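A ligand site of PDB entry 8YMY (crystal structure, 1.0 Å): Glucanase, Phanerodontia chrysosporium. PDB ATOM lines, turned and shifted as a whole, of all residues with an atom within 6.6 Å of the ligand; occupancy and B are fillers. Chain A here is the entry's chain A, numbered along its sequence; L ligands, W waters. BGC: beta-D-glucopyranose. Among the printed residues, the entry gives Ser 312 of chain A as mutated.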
ATOM      1  N   TYR A  16      18.908 -21.486   9.771  1.00  0.00           N
ATOM      2  CA  TYR A  16      19.159 -22.637  10.621  1.00  0.00           C
ATOM      3  C   TYR A  16      18.422 -23.865  10.094  1.00  0.00           C
ATOM      4  O   TYR A  16      19.006 -24.943   9.919  1.00  0.00           O
ATOM      5  CB  TYR A  16      18.705 -22.294  12.038  1.00  0.00           C
ATOM      6  CG  TYR A  16      18.995 -23.323  13.103  1.00  0.00           C
ATOM      7  CD1 TYR A  16      18.118 -24.369  13.344  1.00  0.00           C
ATOM      8  CD2 TYR A  16      20.121 -23.208  13.911  1.00  0.00           C
ATOM      9  CE1 TYR A  16      18.354 -25.280  14.336  1.00  0.00           C
ATOM     10  CE2 TYR A  16      20.372 -24.128  14.908  1.00  0.00           C
ATOM     11  CZ  TYR A  16      19.492 -25.158  15.120  1.00  0.00           C
ATOM     12  OH  TYR A  16      19.744 -26.053  16.134  1.00  0.00           O
ATOM     13  N   TRP A  48      13.988 -21.127  16.639  1.00  0.00           N
ATOM     14  CA  TRP A  48      13.810 -21.158  18.086  1.00  0.00           C
ATOM     15  C   TRP A  48      15.072 -20.678  18.790  1.00  0.00           C
ATOM     16  O   TRP A  48      16.175 -21.186  18.544  1.00  0.00           O
ATOM     17  CB  TRP A  48      13.451 -22.559  18.550  1.00  0.00           C
ATOM     18  CG  TRP A  48      12.106 -23.013  18.125  1.00  0.00           C
ATOM     19  CD1 TRP A  48      11.616 -23.072  16.840  1.00  0.00           C
ATOM     20  CD2 TRP A  48      11.071 -23.524  18.973  1.00  0.00           C
ATOM     21  NE1 TRP A  48      10.335 -23.559  16.856  1.00  0.00           N
ATOM     22  CE2 TRP A  48       9.985 -23.860  18.147  1.00  0.00           C
ATOM     23  CE3 TRP A  48      10.956 -23.735  20.353  1.00  0.00           C
ATOM     24  CZ2 TRP A  48       8.801 -24.396  18.649  1.00  0.00           C
ATOM     25  CZ3 TRP A  48       9.793 -24.252  20.847  1.00  0.00           C
ATOM     26  CH2 TRP A  48       8.726 -24.576  20.002  1.00  0.00           C
ATOM     27  N   LEU A  49      14.893 -19.702  19.680  1.00  0.00           N
ATOM     28  CA  LEU A  49      15.964 -19.262  20.563  1.00  0.00           C
ATOM     29  C   LEU A  49      15.864 -20.088  21.849  1.00  0.00           C
ATOM     30  O   LEU A  49      15.453 -19.629  22.912  1.00  0.00           O
ATOM     31  CB  LEU A  49      15.898 -17.763  20.787  1.00  0.00           C
ATOM     32  CG  LEU A  49      15.849 -16.941  19.491  1.00  0.00           C
ATOM     33  CD1 LEU A  49      15.875 -15.457  19.805  1.00  0.00           C
ATOM     34  CD2 LEU A  49      16.957 -17.310  18.519  1.00  0.00           C
ATOM     35  N   ASP A  50      16.222 -21.376  21.707  1.00  0.00           N
ATOM     36  CA  ASP A  50      16.053 -22.348  22.781  1.00  0.00           C
ATOM     37  C   ASP A  50      17.225 -22.366  23.744  1.00  0.00           C
ATOM     38  O   ASP A  50      17.198 -23.141  24.704  1.00  0.00           O
ATOM     39  CB  ASP A  50      15.786 -23.748  22.207  1.00  0.00           C
ATOM     40  CG  ASP A  50      16.938 -24.283  21.361  1.00  0.00           C
ATOM     41  OD1 ASP A  50      17.489 -23.510  20.549  1.00  0.00           O
ATOM     42  OD2 ASP A  50      17.264 -25.476  21.505  1.00  0.00           O
ATOM     43  N   LYS A  54      21.892 -19.438  20.880  1.00  0.00           N
ATOM     44  CA  LYS A  54      21.207 -19.033  19.667  1.00  0.00           C
ATOM     45  C   LYS A  54      21.089 -17.520  19.523  1.00  0.00           C
ATOM     46  O   LYS A  54      20.693 -17.045  18.453  1.00  0.00           O
ATOM     47  CB  LYS A  54      19.811 -19.671  19.602  1.00  0.00           C
ATOM     48  CG  LYS A  54      19.801 -21.192  19.744  1.00  0.00           C
ATOM     49  CD  LYS A  54      20.611 -21.880  18.646  1.00  0.00           C
ATOM     50  CE  LYS A  54      20.520 -23.404  18.754  1.00  0.00           C
ATOM     51  NZ  LYS A  54      19.171 -23.910  18.376  1.00  0.00           N
ATOM     52  N   TYR A  83      12.107 -19.281  23.943  1.00  0.00           N
ATOM     53  CA  TYR A  83      11.881 -20.603  24.540  1.00  0.00           C
ATOM     54  C   TYR A  83      13.059 -20.973  25.445  1.00  0.00           C
ATOM     55  O   TYR A  83      13.876 -21.851  25.137  1.00  0.00           O
ATOM     56  CB  TYR A  83      11.661 -21.678  23.476  1.00  0.00           C
ATOM     57  CG  TYR A  83      11.246 -23.024  24.020  1.00  0.00           C
ATOM     58  CD1 TYR A  83      10.079 -23.169  24.768  1.00  0.00           C
ATOM     59  CD2 TYR A  83      12.016 -24.166  23.778  1.00  0.00           C
ATOM     60  CE1 TYR A  83       9.681 -24.398  25.250  1.00  0.00           C
ATOM     61  CE2 TYR A  83      11.619 -25.404  24.266  1.00  0.00           C
ATOM     62  CZ  TYR A  83      10.459 -25.503  25.008  1.00  0.00           C
ATOM     63  OH  TYR A  83      10.075 -26.741  25.495  1.00  0.00           O
ATOM     64  N   ARG A  88      12.020 -25.015  32.402  1.00  0.00           N
ATOM     65  CA  ARG A  88      11.236 -25.128  31.183  1.00  0.00           C
ATOM     66  C   ARG A  88      10.544 -26.483  31.124  1.00  0.00           C
ATOM     67  O   ARG A  88      11.058 -27.491  31.626  1.00  0.00           O
ATOM     68  CB  ARG A  88      12.188 -25.002  29.983  1.00  0.00           C
ATOM     69  CG  ARG A  88      11.536 -24.648  28.664  1.00  0.00           C
ATOM     70  CD  ARG A  88      12.565 -24.337  27.594  1.00  0.00           C
ATOM     71  NE  ARG A  88      13.368 -25.514  27.235  1.00  0.00           N
ATOM     72  CZ  ARG A  88      14.447 -25.483  26.472  1.00  0.00           C
ATOM     73  NH1 ARG A  88      14.890 -24.349  25.941  1.00  0.00           N
ATOM     74  NH2 ARG A  88      15.111 -26.620  26.228  1.00  0.00           N
ATOM     75  N   ALA A  94      10.994 -33.975  28.374  1.00  0.00           N
ATOM     76  CA  ALA A  94      11.786 -34.068  27.157  1.00  0.00           C
ATOM     77  C   ALA A  94      12.550 -32.807  26.811  1.00  0.00           C
ATOM     78  O   ALA A  94      13.579 -32.880  26.130  1.00  0.00           O
ATOM     79  CB  ALA A  94      10.898 -34.501  25.998  1.00  0.00           C
ATOM     80  N   SER A  95      12.064 -31.648  27.226  1.00  0.00           N
ATOM     81  CA  SER A  95      12.614 -30.374  26.776  1.00  0.00           C
ATOM     82  C   SER A  95      13.116 -29.509  27.925  1.00  0.00           C
ATOM     83  O   SER A  95      13.154 -28.274  27.814  1.00  0.00           O
ATOM     84  CB  SER A  95      11.659 -29.619  25.858  1.00  0.00           C
ATOM     85  OG  SER A  95      11.639 -30.241  24.584  1.00  0.00           O
ATOM     86  N   ASN A  96      13.513 -30.130  29.033  1.00  0.00           N
ATOM     87  CA  ASN A  96      14.161 -29.366  30.084  1.00  0.00           C
ATOM     88  C   ASN A  96      15.349 -28.598  29.509  1.00  0.00           C
ATOM     89  O   ASN A  96      16.067 -29.077  28.635  1.00  0.00           O
ATOM     90  CB  ASN A  96      14.594 -30.301  31.217  1.00  0.00           C
ATOM     91  CG  ASN A  96      13.417 -30.961  31.905  1.00  0.00           C
ATOM     92  OD1 ASN A  96      12.286 -30.483  31.823  1.00  0.00           O
ATOM     93  ND2 ASN A  96      13.683 -32.049  32.603  1.00  0.00           N
ATOM     94  N   ALA A 218       4.067 -27.168  17.779  1.00  0.00           N
ATOM     95  CA  ALA A 218       4.646 -28.489  17.985  1.00  0.00           C
ATOM     96  C   ALA A 218       3.586 -29.562  18.166  1.00  0.00           C
ATOM     97  O   ALA A 218       3.885 -30.659  18.646  1.00  0.00           O
ATOM     98  CB  ALA A 218       5.670 -28.506  19.128  1.00  0.00           C
ATOM     99  N   VAL A 306       5.631 -23.238  13.057  1.00  0.00           N
ATOM    100  CA  VAL A 306       6.392 -22.820  14.221  1.00  0.00           C
ATOM    101  C   VAL A 306       7.414 -23.888  14.607  1.00  0.00           C
ATOM    102  O   VAL A 306       8.622 -23.621  14.600  1.00  0.00           O
ATOM    103  CB  VAL A 306       5.510 -22.436  15.435  1.00  0.00           C
ATOM    104  CG1 VAL A 306       6.373 -21.893  16.542  1.00  0.00           C
ATOM    105  CG2 VAL A 306       4.465 -21.430  15.036  1.00  0.00           C
ATOM    106  N   LYS A 307       6.940 -25.091  14.944  1.00  0.00           N
ATOM    107  CA  LYS A 307       7.863 -26.201  15.176  1.00  0.00           C
ATOM    108  C   LYS A 307       8.531 -26.589  13.852  1.00  0.00           C
ATOM    109  O   LYS A 307       7.822 -26.813  12.866  1.00  0.00           O
ATOM    110  CB  LYS A 307       7.090 -27.377  15.741  1.00  0.00           C
ATOM    111  CG  LYS A 307       7.856 -28.701  15.810  1.00  0.00           C
ATOM    112  CD  LYS A 307       8.938 -28.683  16.878  1.00  0.00           C
ATOM    113  CE  LYS A 307       9.718 -29.981  16.865  1.00  0.00           C
ATOM    114  NZ  LYS A 307      10.703 -30.051  17.972  1.00  0.00           N
ATOM    115  N   PRO A 308       9.858 -26.683  13.784  1.00  0.00           N
ATOM    116  CA  PRO A 308      10.501 -27.046  12.515  1.00  0.00           C
ATOM    117  C   PRO A 308      10.466 -28.555  12.352  1.00  0.00           C
ATOM    118  O   PRO A 308      11.182 -29.292  13.041  1.00  0.00           O
ATOM    119  CB  PRO A 308      11.925 -26.500  12.671  1.00  0.00           C
ATOM    120  CG  PRO A 308      11.881 -25.620  13.929  1.00  0.00           C
ATOM    121  CD  PRO A 308      10.867 -26.299  14.783  1.00  0.00           C
ATOM    122  N   GLU A 311      12.986 -31.700  13.522  1.00  0.00           N
ATOM    123  CA  GLU A 311      13.633 -31.593  14.811  1.00  0.00           C
ATOM    124  C   GLU A 311      12.816 -32.377  15.831  1.00  0.00           C
ATOM    125  O   GLU A 311      11.600 -32.189  15.952  1.00  0.00           O
ATOM    126  CB  GLU A 311      13.788 -30.122  15.220  1.00  0.00           C
ATOM    127  CG  GLU A 311      14.719 -29.358  14.284  1.00  0.00           C
ATOM    128  CD  GLU A 311      14.777 -27.872  14.549  1.00  0.00           C
ATOM    129  OE1 GLU A 311      14.280 -27.412  15.603  1.00  0.00           O
ATOM    130  OE2 GLU A 311      15.368 -27.148  13.717  1.00  0.00           O
ATOM    131  N   SER A 312      13.470 -33.289  16.557  1.00  0.00           N
ATOM    132  CA  SER A 312      12.760 -34.210  17.431  1.00  0.00           C
ATOM    133  C   SER A 312      11.956 -33.486  18.511  1.00  0.00           C
ATOM    134  O   SER A 312      12.324 -32.399  18.972  1.00  0.00           O
ATOM    135  CB  SER A 312      13.771 -35.146  18.099  1.00  0.00           C
ATOM    136  OG  SER A 312      13.109 -36.057  18.951  1.00  0.00           O
ATOM    137  N   ASP A 313      10.864 -34.131  18.943  1.00  0.00           N
ATOM    138  CA  ASP A 313      10.083 -33.680  20.089  1.00  0.00           C
ATOM    139  C   ASP A 313      10.627 -34.200  21.409  1.00  0.00           C
ATOM    140  O   ASP A 313      10.188 -33.765  22.475  1.00  0.00           O
ATOM    141  CB  ASP A 313       8.636 -34.167  19.980  1.00  0.00           C
ATOM    142  CG  ASP A 313       7.888 -33.564  18.838  1.00  0.00           C
ATOM    143  OD1 ASP A 313       8.095 -32.367  18.546  1.00  0.00           O
ATOM    144  OD2 ASP A 313       7.071 -34.299  18.229  1.00  0.00           O
ATOM    145  N   GLY A 314      11.537 -35.164  21.367  1.00  0.00           N
ATOM    146  CA  GLY A 314      12.014 -35.792  22.578  1.00  0.00           C
ATOM    147  C   GLY A 314      12.638 -37.145  22.311  1.00  0.00           C
ATOM    148  O   GLY A 314      12.296 -37.829  21.349  1.00  0.00           O
ATOM    149  N   ARG A 322      16.250 -36.659  30.138  1.00  0.00           N
ATOM    150  CA  ARG A 322      15.104 -36.027  29.504  1.00  0.00           C
ATOM    151  C   ARG A 322      14.124 -37.034  28.925  1.00  0.00           C
ATOM    152  O   ARG A 322      13.330 -36.691  28.040  1.00  0.00           O
ATOM    153  CB  ARG A 322      15.574 -35.017  28.463  1.00  0.00           C
ATOM    154  CG  ARG A 322      16.500 -33.960  29.064  1.00  0.00           C
ATOM    155  CD  ARG A 322      16.498 -32.663  28.277  1.00  0.00           C
ATOM    156  NE  ARG A 322      16.827 -32.866  26.874  1.00  0.00           N
ATOM    157  CZ  ARG A 322      16.674 -31.942  25.944  1.00  0.00           C
ATOM    158  NH1 ARG A 322      16.271 -30.717  26.241  1.00  0.00           N
ATOM    159  NH2 ARG A 322      16.898 -32.257  24.668  1.00  0.00           N
ATOM    160  N   ALA A 339      15.250 -34.011  22.111  1.00  0.00           N
ATOM    161  CA  ALA A 339      14.405 -32.930  21.630  1.00  0.00           C
ATOM    162  C   ALA A 339      15.245 -31.821  21.020  1.00  0.00           C
ATOM    163  O   ALA A 339      16.268 -31.415  21.589  1.00  0.00           O
ATOM    164  CB  ALA A 339      13.570 -32.363  22.785  1.00  0.00           C
ATOM    165  N   GLY A 340      14.800 -31.331  19.872  1.00  0.00           N
ATOM    166  CA  GLY A 340      15.447 -30.263  19.152  1.00  0.00           C
ATOM    167  C   GLY A 340      16.489 -30.726  18.175  1.00  0.00           C
ATOM    168  O   GLY A 340      16.802 -29.985  17.233  1.00  0.00           O
ATOM    169  N   THR A 341      17.031 -31.919  18.353  1.00  0.00           N
ATOM    170  CA  THR A 341      18.050 -32.414  17.437  1.00  0.00           C
ATOM    171  C   THR A 341      17.424 -33.079  16.213  1.00  0.00           C
ATOM    172  O   THR A 341      16.272 -33.502  16.224  1.00  0.00           O
ATOM    173  CB  THR A 341      19.049 -33.349  18.123  1.00  0.00           C
ATOM    174  OG1 THR A 341      18.446 -34.630  18.362  1.00  0.00           O
ATOM    175  CG2 THR A 341      19.554 -32.755  19.444  1.00  0.00           C
HETATM  176  C2  BGC L   1      13.241 -28.458  21.773  1.00  0.00           C
HETATM  177  C3  BGC L   1      14.013 -27.264  21.353  1.00  0.00           C
HETATM  178  C4  BGC L   1      13.805 -26.891  19.909  1.00  0.00           C
HETATM  179  C5  BGC L   1      12.312 -26.861  19.529  1.00  0.00           C
HETATM  180  C6  BGC L   1      12.098 -26.750  18.050  1.00  0.00           C
HETATM  181  C1  BGC L   1      11.779 -28.305  21.405  1.00  0.00           C
HETATM  182  O1  BGC L   1      11.081 -29.421  21.690  1.00  0.00           O
HETATM  183  O2  BGC L   1      13.322 -28.626  23.200  1.00  0.00           O
HETATM  184  O3  BGC L   1      15.417 -27.520  21.634  1.00  0.00           O
HETATM  185  O4  BGC L   1      14.346 -25.597  19.692  1.00  0.00           O
HETATM  186  O5  BGC L   1      11.659 -28.093  19.940  1.00  0.00           O
HETATM  187  O6  BGC L   1      12.453 -27.969  17.426  1.00  0.00           O
HETATM  188  O   HOH W   1      15.500 -25.569  17.174  1.00  0.00           O
HETATM  189  O   HOH W   2      15.870 -29.126  24.121  1.00  0.00           O
HETATM  190  O   HOH W   3       9.100 -28.463  23.443  1.00  0.00           O
HETATM  191  O   HOH W   4      17.245 -26.581  24.150  1.00  0.00           O
HETATM  192  O   HOH W   5       8.844 -30.252  20.047  1.00  0.00           O
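Residues that only touch the ligand: Trp 48 (3.4 Å), Tyr 83 (3.8 Å), Pro 308 (3.5 Å), Ala 339 (3.8 Å) and Gly 340 (3.7 Å).
Hydrophobic or aromatic side chains that line the ligand: Trp 48, Tyr 83, Pro 308 and Ala 339.
Within 4 Å of the ligand: Trp 48, Asp 50, Tyr 83, Ser 95, Lys 307, Pro 308, Glu 311, Ala 339 and Gly 340.
Water W2 lies within hydrogen-bond range of NH1 of Arg 322, O2 of the ligand, NH2 of Arg 88 and O of Ala 339.
Water W1 lies within hydrogen-bond range of OE1 of Glu 311 (2.7 Å) and O4 of the ligand (2.8 Å).
Water W3 lies within hydrogen-bond range of O1 of the ligand (2.8 Å), OH of Tyr 83 (2.9 Å) and OG of Ser 95 (3.3 Å).
Water W5 lies within hydrogen-bond range of the side-chain carboxylate of Asp 313, the side-chain amino group of Lys 307 and an oxygen (O1) of the ligand.
Water W4 lies within hydrogen-bond range of OD2 of Asp 50 (2.9 Å), NH2 of Arg 88 (3.0 Å) and O3 of the ligand (3.2 Å).
An oxygen (O6) of the ligand is in hydrogen-bond range of the side-chain carboxylate of Glu 311, at 2.6 Å.
An oxygen (O2) of the ligand is in hydrogen-bond range of the side-chain hydroxyl of Ser 95 (2.7 Å).
The side-chain carboxylate (OD2) of Asp 50 is in hydrogen-bond range of an oxygen (O3) of the ligand.
The side-chain amino group of Lys 307 sits at hydrogen-bond distance from an oxygen (O6) of the ligand (2.8 Å).
The backbone carbonyl oxygen (O) of Ser 95 sits at hydrogen-bond distance from the guanidinium group (NE) of Arg 88 (2.8 Å).
NH1 of Arg 88 sits at hydrogen-bond distance from O of Asp 50.
NZ of Lys 54 lies within salt-bridge range of OD1 of Asp 50 (2.8 Å).
The side-chain amino group (NZ) of Lys 307 sits at hydrogen-bond distance from the backbone carbonyl oxygen (O) of Ser 312.
The side-chain amino group (NZ) of Lys 307 lies within salt-bridge range of the side-chain carboxylate (OD1) of Asp 313, at 3.5 Å.
The indole nitrogen (NE1) of Trp 48 is in hydrogen-bond range of the backbone carbonyl oxygen (O) of Val 306 (2.8 Å).
The backbone carbonyl oxygen of Ser 312 is in hydrogen-bond range of the backbone NH of Gly 340.
The backbone carbonyl oxygen of Ala 339 is in hydrogen-bond range of the guanidinium group of Arg 322 (3.3 Å).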
